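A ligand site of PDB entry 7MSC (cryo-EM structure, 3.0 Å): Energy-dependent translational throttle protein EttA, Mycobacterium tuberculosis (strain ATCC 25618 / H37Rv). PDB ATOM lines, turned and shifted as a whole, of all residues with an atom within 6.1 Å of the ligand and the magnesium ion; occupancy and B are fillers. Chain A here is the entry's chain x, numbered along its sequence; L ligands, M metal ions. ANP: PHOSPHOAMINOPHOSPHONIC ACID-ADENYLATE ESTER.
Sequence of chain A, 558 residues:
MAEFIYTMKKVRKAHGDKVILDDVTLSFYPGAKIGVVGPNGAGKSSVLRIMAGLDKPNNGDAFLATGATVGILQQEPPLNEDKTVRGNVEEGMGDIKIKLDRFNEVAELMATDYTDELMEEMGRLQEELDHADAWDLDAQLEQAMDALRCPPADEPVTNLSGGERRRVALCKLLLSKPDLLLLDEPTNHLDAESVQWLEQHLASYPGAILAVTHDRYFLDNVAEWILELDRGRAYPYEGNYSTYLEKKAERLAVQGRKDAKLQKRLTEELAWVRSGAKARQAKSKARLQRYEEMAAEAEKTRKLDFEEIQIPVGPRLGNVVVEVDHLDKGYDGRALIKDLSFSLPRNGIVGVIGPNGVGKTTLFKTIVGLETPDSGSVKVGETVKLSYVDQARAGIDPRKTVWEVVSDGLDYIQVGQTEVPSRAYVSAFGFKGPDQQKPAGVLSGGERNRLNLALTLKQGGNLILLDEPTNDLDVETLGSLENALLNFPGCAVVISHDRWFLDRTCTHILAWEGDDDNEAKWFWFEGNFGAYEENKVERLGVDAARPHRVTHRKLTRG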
ATOM      1  N   ASN A 159      11.292 -17.472 -13.997  1.00  0.00           N
ATOM      2  CA  ASN A 159       9.852 -17.199 -14.001  1.00  0.00           C
ATOM      3  C   ASN A 159       9.563 -15.699 -14.034  1.00  0.00           C
ATOM      4  O   ASN A 159       8.827 -15.177 -13.209  1.00  0.00           O
ATOM      5  CB  ASN A 159       9.193 -17.848 -12.800  1.00  0.00           C
ATOM      6  CG  ASN A 159       9.177 -19.356 -12.906  1.00  0.00           C
ATOM      7  OD1 ASN A 159       8.951 -19.912 -13.971  1.00  0.00           O
ATOM      8  ND2 ASN A 159       9.406 -20.029 -11.782  1.00  0.00           N
ATOM      9  N   LEU A 160      10.161 -15.006 -14.998  1.00  0.00           N
ATOM     10  CA  LEU A 160       9.889 -13.594 -15.216  1.00  0.00           C
ATOM     11  C   LEU A 160       9.046 -13.419 -16.467  1.00  0.00           C
ATOM     12  O   LEU A 160       8.710 -14.378 -17.175  1.00  0.00           O
ATOM     13  CB  LEU A 160      11.174 -12.780 -15.308  1.00  0.00           C
ATOM     14  CG  LEU A 160      11.945 -12.542 -14.025  1.00  0.00           C
ATOM     15  CD1 LEU A 160      13.237 -11.820 -14.342  1.00  0.00           C
ATOM     16  CD2 LEU A 160      11.104 -11.721 -13.080  1.00  0.00           C
ATOM     17  N   SER A 161       8.724 -12.163 -16.763  1.00  0.00           N
ATOM     18  CA  SER A 161       7.906 -11.816 -17.902  1.00  0.00           C
ATOM     19  C   SER A 161       8.740 -11.817 -19.172  1.00  0.00           C
ATOM     20  O   SER A 161       9.869 -12.309 -19.210  1.00  0.00           O
ATOM     21  CB  SER A 161       7.242 -10.470 -17.677  1.00  0.00           C
ATOM     22  OG  SER A 161       6.374 -10.503 -16.555  1.00  0.00           O
ATOM     23  N   GLY A 162       8.190 -11.272 -20.249  1.00  0.00           N
ATOM     24  CA  GLY A 162       8.975 -11.019 -21.429  1.00  0.00           C
ATOM     25  C   GLY A 162       9.531  -9.611 -21.394  1.00  0.00           C
ATOM     26  O   GLY A 162      10.554  -9.312 -22.020  1.00  0.00           O
ATOM     27  N   GLY A 163       8.862  -8.745 -20.639  1.00  0.00           N
ATOM     28  CA  GLY A 163       9.284  -7.367 -20.524  1.00  0.00           C
ATOM     29  C   GLY A 163      10.107  -7.148 -19.288  1.00  0.00           C
ATOM     30  O   GLY A 163      10.917  -6.213 -19.216  1.00  0.00           O
ATOM     31  N   GLU A 164       9.917  -8.002 -18.287  1.00  0.00           N
ATOM     32  CA  GLU A 164      10.769  -7.967 -17.107  1.00  0.00           C
ATOM     33  C   GLU A 164      12.155  -8.521 -17.404  1.00  0.00           C
ATOM     34  O   GLU A 164      13.105  -8.174 -16.708  1.00  0.00           O
ATOM     35  CB  GLU A 164      10.108  -8.752 -15.978  1.00  0.00           C
ATOM     36  CG  GLU A 164       8.886  -8.057 -15.420  1.00  0.00           C
ATOM     37  CD  GLU A 164       8.120  -8.922 -14.443  1.00  0.00           C
ATOM     38  OE1 GLU A 164       8.453 -10.118 -14.325  1.00  0.00           O
ATOM     39  OE2 GLU A 164       7.187  -8.405 -13.795  1.00  0.00           O
ATOM     40  N   HIS A 189       8.838  -5.646 -26.095  1.00  0.00           N
ATOM     41  CA  HIS A 189       8.218  -6.210 -24.892  1.00  0.00           C
ATOM     42  C   HIS A 189       7.967  -5.208 -23.776  1.00  0.00           C
ATOM     43  O   HIS A 189       7.485  -5.598 -22.710  1.00  0.00           O
ATOM     44  CB  HIS A 189       9.045  -7.369 -24.345  1.00  0.00           C
ATOM     45  CG  HIS A 189       9.310  -8.460 -25.338  1.00  0.00           C
ATOM     46  ND1 HIS A 189       8.313  -9.261 -25.844  1.00  0.00           N
ATOM     47  CD2 HIS A 189      10.472  -8.918 -25.866  1.00  0.00           C
ATOM     48  CE1 HIS A 189       8.847 -10.146 -26.672  1.00  0.00           C
ATOM     49  NE2 HIS A 189      10.152  -9.958 -26.693  1.00  0.00           N
ATOM     50  N   TYR A 331       0.089 -17.095  -8.436  1.00  0.00           N
ATOM     51  CA  TYR A 331       1.220 -17.983  -8.178  1.00  0.00           C
ATOM     52  C   TYR A 331       1.678 -17.978  -6.727  1.00  0.00           C
ATOM     53  O   TYR A 331       2.313 -18.933  -6.294  1.00  0.00           O
ATOM     54  CB  TYR A 331       2.392 -17.596  -9.075  1.00  0.00           C
ATOM     55  CG  TYR A 331       2.146 -17.900 -10.527  1.00  0.00           C
ATOM     56  CD1 TYR A 331       2.324 -19.178 -11.021  1.00  0.00           C
ATOM     57  CD2 TYR A 331       1.724 -16.906 -11.398  1.00  0.00           C
ATOM     58  CE1 TYR A 331       2.101 -19.463 -12.348  1.00  0.00           C
ATOM     59  CE2 TYR A 331       1.498 -17.179 -12.728  1.00  0.00           C
ATOM     60  CZ  TYR A 331       1.689 -18.455 -13.195  1.00  0.00           C
ATOM     61  OH  TYR A 331       1.470 -18.754 -14.519  1.00  0.00           O
ATOM     62  N   ASP A 332       1.348 -16.929  -5.989  1.00  0.00           N
ATOM     63  CA  ASP A 332       1.719 -16.733  -4.593  1.00  0.00           C
ATOM     64  C   ASP A 332       0.576 -15.955  -3.946  1.00  0.00           C
ATOM     65  O   ASP A 332      -0.554 -15.975  -4.446  1.00  0.00           O
ATOM     66  CB  ASP A 332       3.066 -16.012  -4.463  1.00  0.00           C
ATOM     67  CG  ASP A 332       4.243 -16.937  -4.696  1.00  0.00           C
ATOM     68  OD1 ASP A 332       4.167 -18.113  -4.311  1.00  0.00           O
ATOM     69  OD2 ASP A 332       5.258 -16.468  -5.250  1.00  0.00           O
ATOM     70  N   ARG A 334       0.387 -12.883  -4.117  1.00  0.00           N
ATOM     71  CA  ARG A 334       0.019 -11.956  -5.179  1.00  0.00           C
ATOM     72  C   ARG A 334      -1.075 -12.561  -6.045  1.00  0.00           C
ATOM     73  O   ARG A 334      -0.992 -13.729  -6.442  1.00  0.00           O
ATOM     74  CB  ARG A 334       1.244 -11.630  -6.042  1.00  0.00           C
ATOM     75  CG  ARG A 334       0.983 -10.607  -7.127  1.00  0.00           C
ATOM     76  CD  ARG A 334       2.201 -10.353  -7.967  1.00  0.00           C
ATOM     77  NE  ARG A 334       1.910  -9.417  -9.043  1.00  0.00           N
ATOM     78  CZ  ARG A 334       2.773  -9.072  -9.991  1.00  0.00           C
ATOM     79  NH1 ARG A 334       3.983  -9.606 -10.004  1.00  0.00           N
ATOM     80  NH2 ARG A 334       2.422  -8.204 -10.934  1.00  0.00           N
ATOM     81  N   LEU A 336      -3.281 -12.106  -9.629  1.00  0.00           N
ATOM     82  CA  LEU A 336      -3.240 -11.492 -10.947  1.00  0.00           C
ATOM     83  C   LEU A 336      -4.627 -11.235 -11.526  1.00  0.00           C
ATOM     84  O   LEU A 336      -4.905 -10.147 -12.024  1.00  0.00           O
ATOM     85  CB  LEU A 336      -2.434 -12.355 -11.913  1.00  0.00           C
ATOM     86  CG  LEU A 336      -0.962 -12.530 -11.565  1.00  0.00           C
ATOM     87  CD1 LEU A 336      -0.294 -13.430 -12.579  1.00  0.00           C
ATOM     88  CD2 LEU A 336      -0.277 -11.187 -11.493  1.00  0.00           C
ATOM     89  N   GLY A 354      -2.284  -4.200 -21.046  1.00  0.00           N
ATOM     90  CA  GLY A 354      -1.770  -4.168 -19.707  1.00  0.00           C
ATOM     91  C   GLY A 354      -0.300  -3.843 -19.655  1.00  0.00           C
ATOM     92  O   GLY A 354       0.449  -4.120 -20.600  1.00  0.00           O
ATOM     93  N   PRO A 355       0.160  -3.273 -18.551  1.00  0.00           N
ATOM     94  CA  PRO A 355       1.596  -3.063 -18.374  1.00  0.00           C
ATOM     95  C   PRO A 355       2.329  -4.345 -18.043  1.00  0.00           C
ATOM     96  O   PRO A 355       1.739  -5.426 -18.007  1.00  0.00           O
ATOM     97  CB  PRO A 355       1.659  -2.064 -17.213  1.00  0.00           C
ATOM     98  CG  PRO A 355       0.395  -2.285 -16.475  1.00  0.00           C
ATOM     99  CD  PRO A 355      -0.629  -2.623 -17.490  1.00  0.00           C
ATOM    100  N   ASN A 356       3.638  -4.241 -17.803  1.00  0.00           N
ATOM    101  CA  ASN A 356       4.466  -5.431 -17.672  1.00  0.00           C
ATOM    102  C   ASN A 356       4.251  -6.129 -16.339  1.00  0.00           C
ATOM    103  O   ASN A 356       4.133  -5.497 -15.293  1.00  0.00           O
ATOM    104  CB  ASN A 356       5.927  -5.064 -17.861  1.00  0.00           C
ATOM    105  CG  ASN A 356       6.266  -4.751 -19.287  1.00  0.00           C
ATOM    106  OD1 ASN A 356       6.588  -3.627 -19.644  1.00  0.00           O
ATOM    107  ND2 ASN A 356       6.195  -5.772 -20.132  1.00  0.00           N
ATOM    108  N   GLY A 357       4.201  -7.458 -16.405  1.00  0.00           N
ATOM    109  CA  GLY A 357       4.043  -8.278 -15.217  1.00  0.00           C
ATOM    110  C   GLY A 357       2.673  -8.186 -14.595  1.00  0.00           C
ATOM    111  O   GLY A 357       2.546  -7.910 -13.398  1.00  0.00           O
ATOM    112  N   VAL A 358       1.623  -8.400 -15.388  1.00  0.00           N
ATOM    113  CA  VAL A 358       0.284  -8.210 -14.867  1.00  0.00           C
ATOM    114  C   VAL A 358      -0.563  -9.437 -15.212  1.00  0.00           C
ATOM    115  O   VAL A 358      -1.652  -9.627 -14.660  1.00  0.00           O
ATOM    116  CB  VAL A 358      -0.337  -6.911 -15.411  1.00  0.00           C
ATOM    117  CG1 VAL A 358      -0.860  -7.094 -16.821  1.00  0.00           C
ATOM    118  CG2 VAL A 358      -1.376  -6.393 -14.474  1.00  0.00           C
ATOM    119  N   GLY A 359      -0.066 -10.279 -16.110  1.00  0.00           N
ATOM    120  CA  GLY A 359      -0.724 -11.549 -16.349  1.00  0.00           C
ATOM    121  C   GLY A 359      -1.393 -11.752 -17.685  1.00  0.00           C
ATOM    122  O   GLY A 359      -2.382 -12.480 -17.770  1.00  0.00           O
ATOM    123  N   LYS A 360      -0.868 -11.131 -18.731  1.00  0.00           N
ATOM    124  CA  LYS A 360      -1.450 -11.310 -20.056  1.00  0.00           C
ATOM    125  C   LYS A 360      -1.136 -12.682 -20.620  1.00  0.00           C
ATOM    126  O   LYS A 360      -1.988 -13.322 -21.235  1.00  0.00           O
ATOM    127  CB  LYS A 360      -0.941 -10.209 -20.994  1.00  0.00           C
ATOM    128  CG  LYS A 360      -1.323  -8.814 -20.555  1.00  0.00           C
ATOM    129  CD  LYS A 360      -0.861  -7.783 -21.558  1.00  0.00           C
ATOM    130  CE  LYS A 360       0.634  -7.572 -21.512  1.00  0.00           C
ATOM    131  NZ  LYS A 360       1.037  -6.929 -20.249  1.00  0.00           N
ATOM    132  N   THR A 361       0.091 -13.157 -20.417  1.00  0.00           N
ATOM    133  CA  THR A 361       0.492 -14.444 -20.963  1.00  0.00           C
ATOM    134  C   THR A 361      -0.021 -15.600 -20.101  1.00  0.00           C
ATOM    135  O   THR A 361      -0.297 -16.682 -20.622  1.00  0.00           O
ATOM    136  CB  THR A 361       2.015 -14.498 -21.103  1.00  0.00           C
ATOM    137  OG1 THR A 361       2.461 -13.313 -21.765  1.00  0.00           O
ATOM    138  CG2 THR A 361       2.450 -15.679 -21.953  1.00  0.00           C
ATOM    139  N   THR A 362      -0.207 -15.375 -18.797  1.00  0.00           N
ATOM    140  CA  THR A 362      -0.886 -16.379 -17.974  1.00  0.00           C
ATOM    141  C   THR A 362      -2.357 -16.494 -18.319  1.00  0.00           C
ATOM    142  O   THR A 362      -2.959 -17.536 -18.059  1.00  0.00           O
ATOM    143  CB  THR A 362      -0.758 -16.038 -16.491  1.00  0.00           C
ATOM    144  OG1 THR A 362      -1.432 -14.804 -16.224  1.00  0.00           O
ATOM    145  CG2 THR A 362       0.686 -15.919 -16.095  1.00  0.00           C
ATOM    146  N   LEU A 363      -2.947 -15.441 -18.901  1.00  0.00           N
ATOM    147  CA  LEU A 363      -4.333 -15.514 -19.321  1.00  0.00           C
ATOM    148  C   LEU A 363      -4.506 -16.442 -20.513  1.00  0.00           C
ATOM    149  O   LEU A 363      -5.510 -17.141 -20.614  1.00  0.00           O
ATOM    150  CB  LEU A 363      -4.843 -14.104 -19.655  1.00  0.00           C
ATOM    151  CG  LEU A 363      -6.306 -13.976 -20.024  1.00  0.00           C
ATOM    152  CD1 LEU A 363      -7.157 -14.365 -18.847  1.00  0.00           C
ATOM    153  CD2 LEU A 363      -6.591 -12.558 -20.434  1.00  0.00           C
ATOM    154  N   LYS A 365      -2.586 -19.026 -21.028  1.00  0.00           N
ATOM    155  CA  LYS A 365      -2.255 -20.381 -20.619  1.00  0.00           C
ATOM    156  C   LYS A 365      -3.347 -21.026 -19.765  1.00  0.00           C
ATOM    157  O   LYS A 365      -3.257 -22.221 -19.480  1.00  0.00           O
ATOM    158  CB  LYS A 365      -0.920 -20.401 -19.887  1.00  0.00           C
ATOM    159  CG  LYS A 365       0.265 -20.173 -20.810  1.00  0.00           C
ATOM    160  CD  LYS A 365       1.587 -20.404 -20.106  1.00  0.00           C
ATOM    161  CE  LYS A 365       1.933 -19.260 -19.180  1.00  0.00           C
ATOM    162  NZ  LYS A 365       3.294 -19.409 -18.587  1.00  0.00           N
ATOM    163  N   GLU A 371      -2.143 -24.015 -17.900  1.00  0.00           N
ATOM    164  CA  GLU A 371      -2.291 -23.697 -16.490  1.00  0.00           C
ATOM    165  C   GLU A 371      -3.626 -24.234 -15.995  1.00  0.00           C
ATOM    166  O   GLU A 371      -4.359 -24.907 -16.724  1.00  0.00           O
ATOM    167  CB  GLU A 371      -2.171 -22.181 -16.262  1.00  0.00           C
ATOM    168  CG  GLU A 371      -0.777 -21.611 -16.433  1.00  0.00           C
ATOM    169  CD  GLU A 371       0.167 -22.017 -15.327  1.00  0.00           C
ATOM    170  OE1 GLU A 371      -0.308 -22.218 -14.187  1.00  0.00           O
ATOM    171  OE2 GLU A 371       1.375 -22.130 -15.594  1.00  0.00           O
ATOM    172  N   ASP A 467       0.637 -13.870 -29.267  1.00  0.00           N
ATOM    173  CA  ASP A 467       1.303 -13.111 -28.212  1.00  0.00           C
ATOM    174  C   ASP A 467       2.379 -12.268 -28.888  1.00  0.00           C
ATOM    175  O   ASP A 467       3.446 -12.767 -29.231  1.00  0.00           O
ATOM    176  CB  ASP A 467       1.887 -14.032 -27.154  1.00  0.00           C
ATOM    177  CG  ASP A 467       2.285 -13.301 -25.891  1.00  0.00           C
ATOM    178  OD1 ASP A 467       2.093 -12.068 -25.824  1.00  0.00           O
ATOM    179  OD2 ASP A 467       2.795 -13.957 -24.969  1.00  0.00           O
ATOM    180  N   GLU A 468       2.082 -10.976 -29.045  1.00  0.00           N
ATOM    181  CA  GLU A 468       2.906  -9.934 -29.659  1.00  0.00           C
ATOM    182  C   GLU A 468       3.412 -10.314 -31.039  1.00  0.00           C
ATOM    183  O   GLU A 468       4.594 -10.613 -31.206  1.00  0.00           O
ATOM    184  CB  GLU A 468       4.076  -9.583 -28.748  1.00  0.00           C
ATOM    185  CG  GLU A 468       3.646  -8.956 -27.444  1.00  0.00           C
ATOM    186  CD  GLU A 468       4.807  -8.651 -26.529  1.00  0.00           C
ATOM    187  OE1 GLU A 468       5.938  -9.039 -26.874  1.00  0.00           O
ATOM    188  OE2 GLU A 468       4.581  -8.028 -25.473  1.00  0.00           O
ATOM    189  N   ILE A 495      -2.372 -10.019 -27.838  1.00  0.00           N
ATOM    190  CA  ILE A 495      -1.687  -9.255 -26.814  1.00  0.00           C
ATOM    191  C   ILE A 495      -0.686  -8.354 -27.516  1.00  0.00           C
ATOM    192  O   ILE A 495       0.125  -8.835 -28.307  1.00  0.00           O
ATOM    193  CB  ILE A 495      -0.972 -10.169 -25.804  1.00  0.00           C
ATOM    194  CG1 ILE A 495      -1.967 -10.997 -25.013  1.00  0.00           C
ATOM    195  CG2 ILE A 495      -0.095  -9.373 -24.879  1.00  0.00           C
ATOM    196  CD1 ILE A 495      -1.294 -12.052 -24.193  1.00  0.00           C
ATOM    197  N   HIS A 497       1.599  -4.283 -27.207  1.00  0.00           N
ATOM    198  CA  HIS A 497       1.890  -2.979 -26.636  1.00  0.00           C
ATOM    199  C   HIS A 497       1.984  -1.900 -27.693  1.00  0.00           C
ATOM    200  O   HIS A 497       2.051  -0.720 -27.339  1.00  0.00           O
ATOM    201  CB  HIS A 497       3.206  -3.015 -25.856  1.00  0.00           C
ATOM    202  CG  HIS A 497       3.192  -3.937 -24.681  1.00  0.00           C
ATOM    203  ND1 HIS A 497       2.552  -3.628 -23.509  1.00  0.00           N
ATOM    204  CD2 HIS A 497       3.738  -5.165 -24.511  1.00  0.00           C
ATOM    205  CE1 HIS A 497       2.709  -4.623 -22.658  1.00  0.00           C
ATOM    206  NE2 HIS A 497       3.419  -5.569 -23.246  1.00  0.00           N
HETATM  207  PG  ANP L   1       4.557  -8.869 -20.488  1.00  0.00           P
HETATM  208  O1G ANP L   1       3.880  -7.568 -20.727  1.00  0.00           O
HETATM  209  O2G ANP L   1       6.101  -8.692 -20.721  1.00  0.00           O
HETATM  210  O3G ANP L   1       4.011  -9.989 -21.461  1.00  0.00           O
HETATM  211  PB  ANP L   1       3.264 -10.670 -18.948  1.00  0.00           P
HETATM  212  O1B ANP L   1       1.934 -10.217 -19.407  1.00  0.00           O
HETATM  213  O2B ANP L   1       3.820 -11.725 -19.933  1.00  0.00           O
HETATM  214  N3B ANP L   1       4.285  -9.338 -18.898  1.00  0.00           N
HETATM  215  PA  ANP L   1       3.134 -12.826 -17.333  1.00  0.00           P
HETATM  216  O1A ANP L   1       4.210 -13.507 -18.076  1.00  0.00           O
HETATM  217  O2A ANP L   1       1.750 -13.275 -17.776  1.00  0.00           O
HETATM  218  O3A ANP L   1       3.147 -11.273 -17.528  1.00  0.00           O
HETATM  219  O5' ANP L   1       3.336 -13.002 -15.784  1.00  0.00           O
HETATM  220  C5' ANP L   1       2.841 -11.989 -14.886  1.00  0.00           C
HETATM  221  C4' ANP L   1       3.456 -12.134 -13.519  1.00  0.00           C
HETATM  222  O4' ANP L   1       3.464 -13.526 -13.121  1.00  0.00           O
HETATM  223  C3' ANP L   1       4.890 -11.641 -13.374  1.00  0.00           C
HETATM  224  O3' ANP L   1       5.061 -11.030 -12.101  1.00  0.00           O
HETATM  225  C2' ANP L   1       5.705 -12.936 -13.465  1.00  0.00           C
HETATM  226  O2' ANP L   1       6.941 -12.815 -12.763  1.00  0.00           O
HETATM  227  C1' ANP L   1       4.779 -13.907 -12.760  1.00  0.00           C
HETATM  228  N9  ANP L   1       4.955 -15.293 -13.133  1.00  0.00           N
HETATM  229  C8  ANP L   1       4.868 -15.824 -14.404  1.00  0.00           C
HETATM  230  N7  ANP L   1       5.063 -17.119 -14.453  1.00  0.00           N
HETATM  231  C5  ANP L   1       5.287 -17.473 -13.128  1.00  0.00           C
HETATM  232  C6  ANP L   1       5.564 -18.701 -12.520  1.00  0.00           C
HETATM  233  N6  ANP L   1       5.655 -19.858 -13.179  1.00  0.00           N
HETATM  234  N1  ANP L   1       5.733 -18.716 -11.177  1.00  0.00           N
HETATM  235  C2  ANP L   1       5.652 -17.556 -10.515  1.00  0.00           C
HETATM  236  N3  ANP L   1       5.391 -16.338 -10.981  1.00  0.00           N
HETATM  237  C4  ANP L   1       5.222 -16.367 -12.318  1.00  0.00           C
HETATM  238 MG    MG M   1       4.165 -12.040 -22.028  1.00  0.00          MG
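An oxygen (O2A) of the ligand sits at hydrogen-bond distance from the backbone NH (N) of Thr 361 (3.1 Å). An oxygen (O3') of the ligand is in hydrogen-bond range of the guanidinium group (NH1) of Arg 334. O2G of the ligand is in hydrogen-bond range of N of Gly 163, 2.8 Å away. The backbone NH (N) of Lys 360 sits at hydrogen-bond distance from an oxygen (O1B) of the ligand. NZ of Lys 360 is in salt-bridge range of O1G of the ligand. The side-chain amide nitrogen of Asn 356 lies within hydrogen-bond range of an oxygen (O2G) of the ligand (3.0 Å). N of Thr 362 sits at hydrogen-bond distance from O2A of the ligand, 3.0 Å away. O of Asn 159 lies within hydrogen-bond range of O2' of the ligand (3.1 Å). OD1 of Asn 159 is in hydrogen-bond range of N6 of the ligand. A ring nitrogen (NE2) of His 497 lies within hydrogen-bond range of an oxygen (O1G) of the ligand (3.2 Å). OG of Ser 161 is in hydrogen-bond range of N3B of the ligand (3.3 Å). An oxygen (O2G) of the ligand lies within hydrogen-bond range of the backbone NH (N) of Gly 162, at 3.4 Å. The side-chain carboxylate (OE1) of Glu 164 sits at hydrogen-bond distance from an oxygen (O2') of the ligand.
OG1 of Thr 361 lies close to OD2 of Asp 467, 3.3 Å away. The guanidinium group of Arg 334 sits at hydrogen-bond distance from the backbone carbonyl oxygen of Gly 357 (2.5 Å). The side-chain amino group of Lys 360 is in hydrogen-bond range of the backbone carbonyl oxygen of Pro 355 (2.8 Å). NZ of Lys 360 sits at hydrogen-bond distance from O of Gly 354, 2.9 Å away. O of His 189 sits at hydrogen-bond distance from ND2 of Asn 356 (2.9 Å). The side-chain hydroxyl (OG1) of Thr 362 lies within hydrogen-bond range of the backbone carbonyl oxygen (O) of Gly 359, 2.9 Å away. OG of Ser 161 is in hydrogen-bond range of OE1 of Glu 164 (3.1 Å). ND1 of His 189 sits at hydrogen-bond distance from OE1 of Glu 468.
A nitrogen (N3B) of the ligand lies close to the backbone NH of Gly 357 (3.1 Å). Residues that only touch the ligand: Gly 359 (3.3 Å), Tyr 331 (3.4 Å), Leu 336 (3.8 Å), Val 358 (3.8 Å), Leu 160 (3.9 Å) and His 189 (3.9 Å). Hydrophobic or aromatic side chains within 4 Å of the ligand: Tyr 331, Leu 336 and His 497. Of the 27 residues printed, 18 come within 4 Å of the ligand. Along chain A the residues within 4 Å of the ligand span positions 159 to 497.
OD2 of Asp 467 touches the magnesium ion, 3.8 Å away.
The magnesium ion is bound by O3G of the ligand (2.1 Å), OG1 of Thr 361 (2.1 Å) and O2B of the ligand (2.1 Å).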
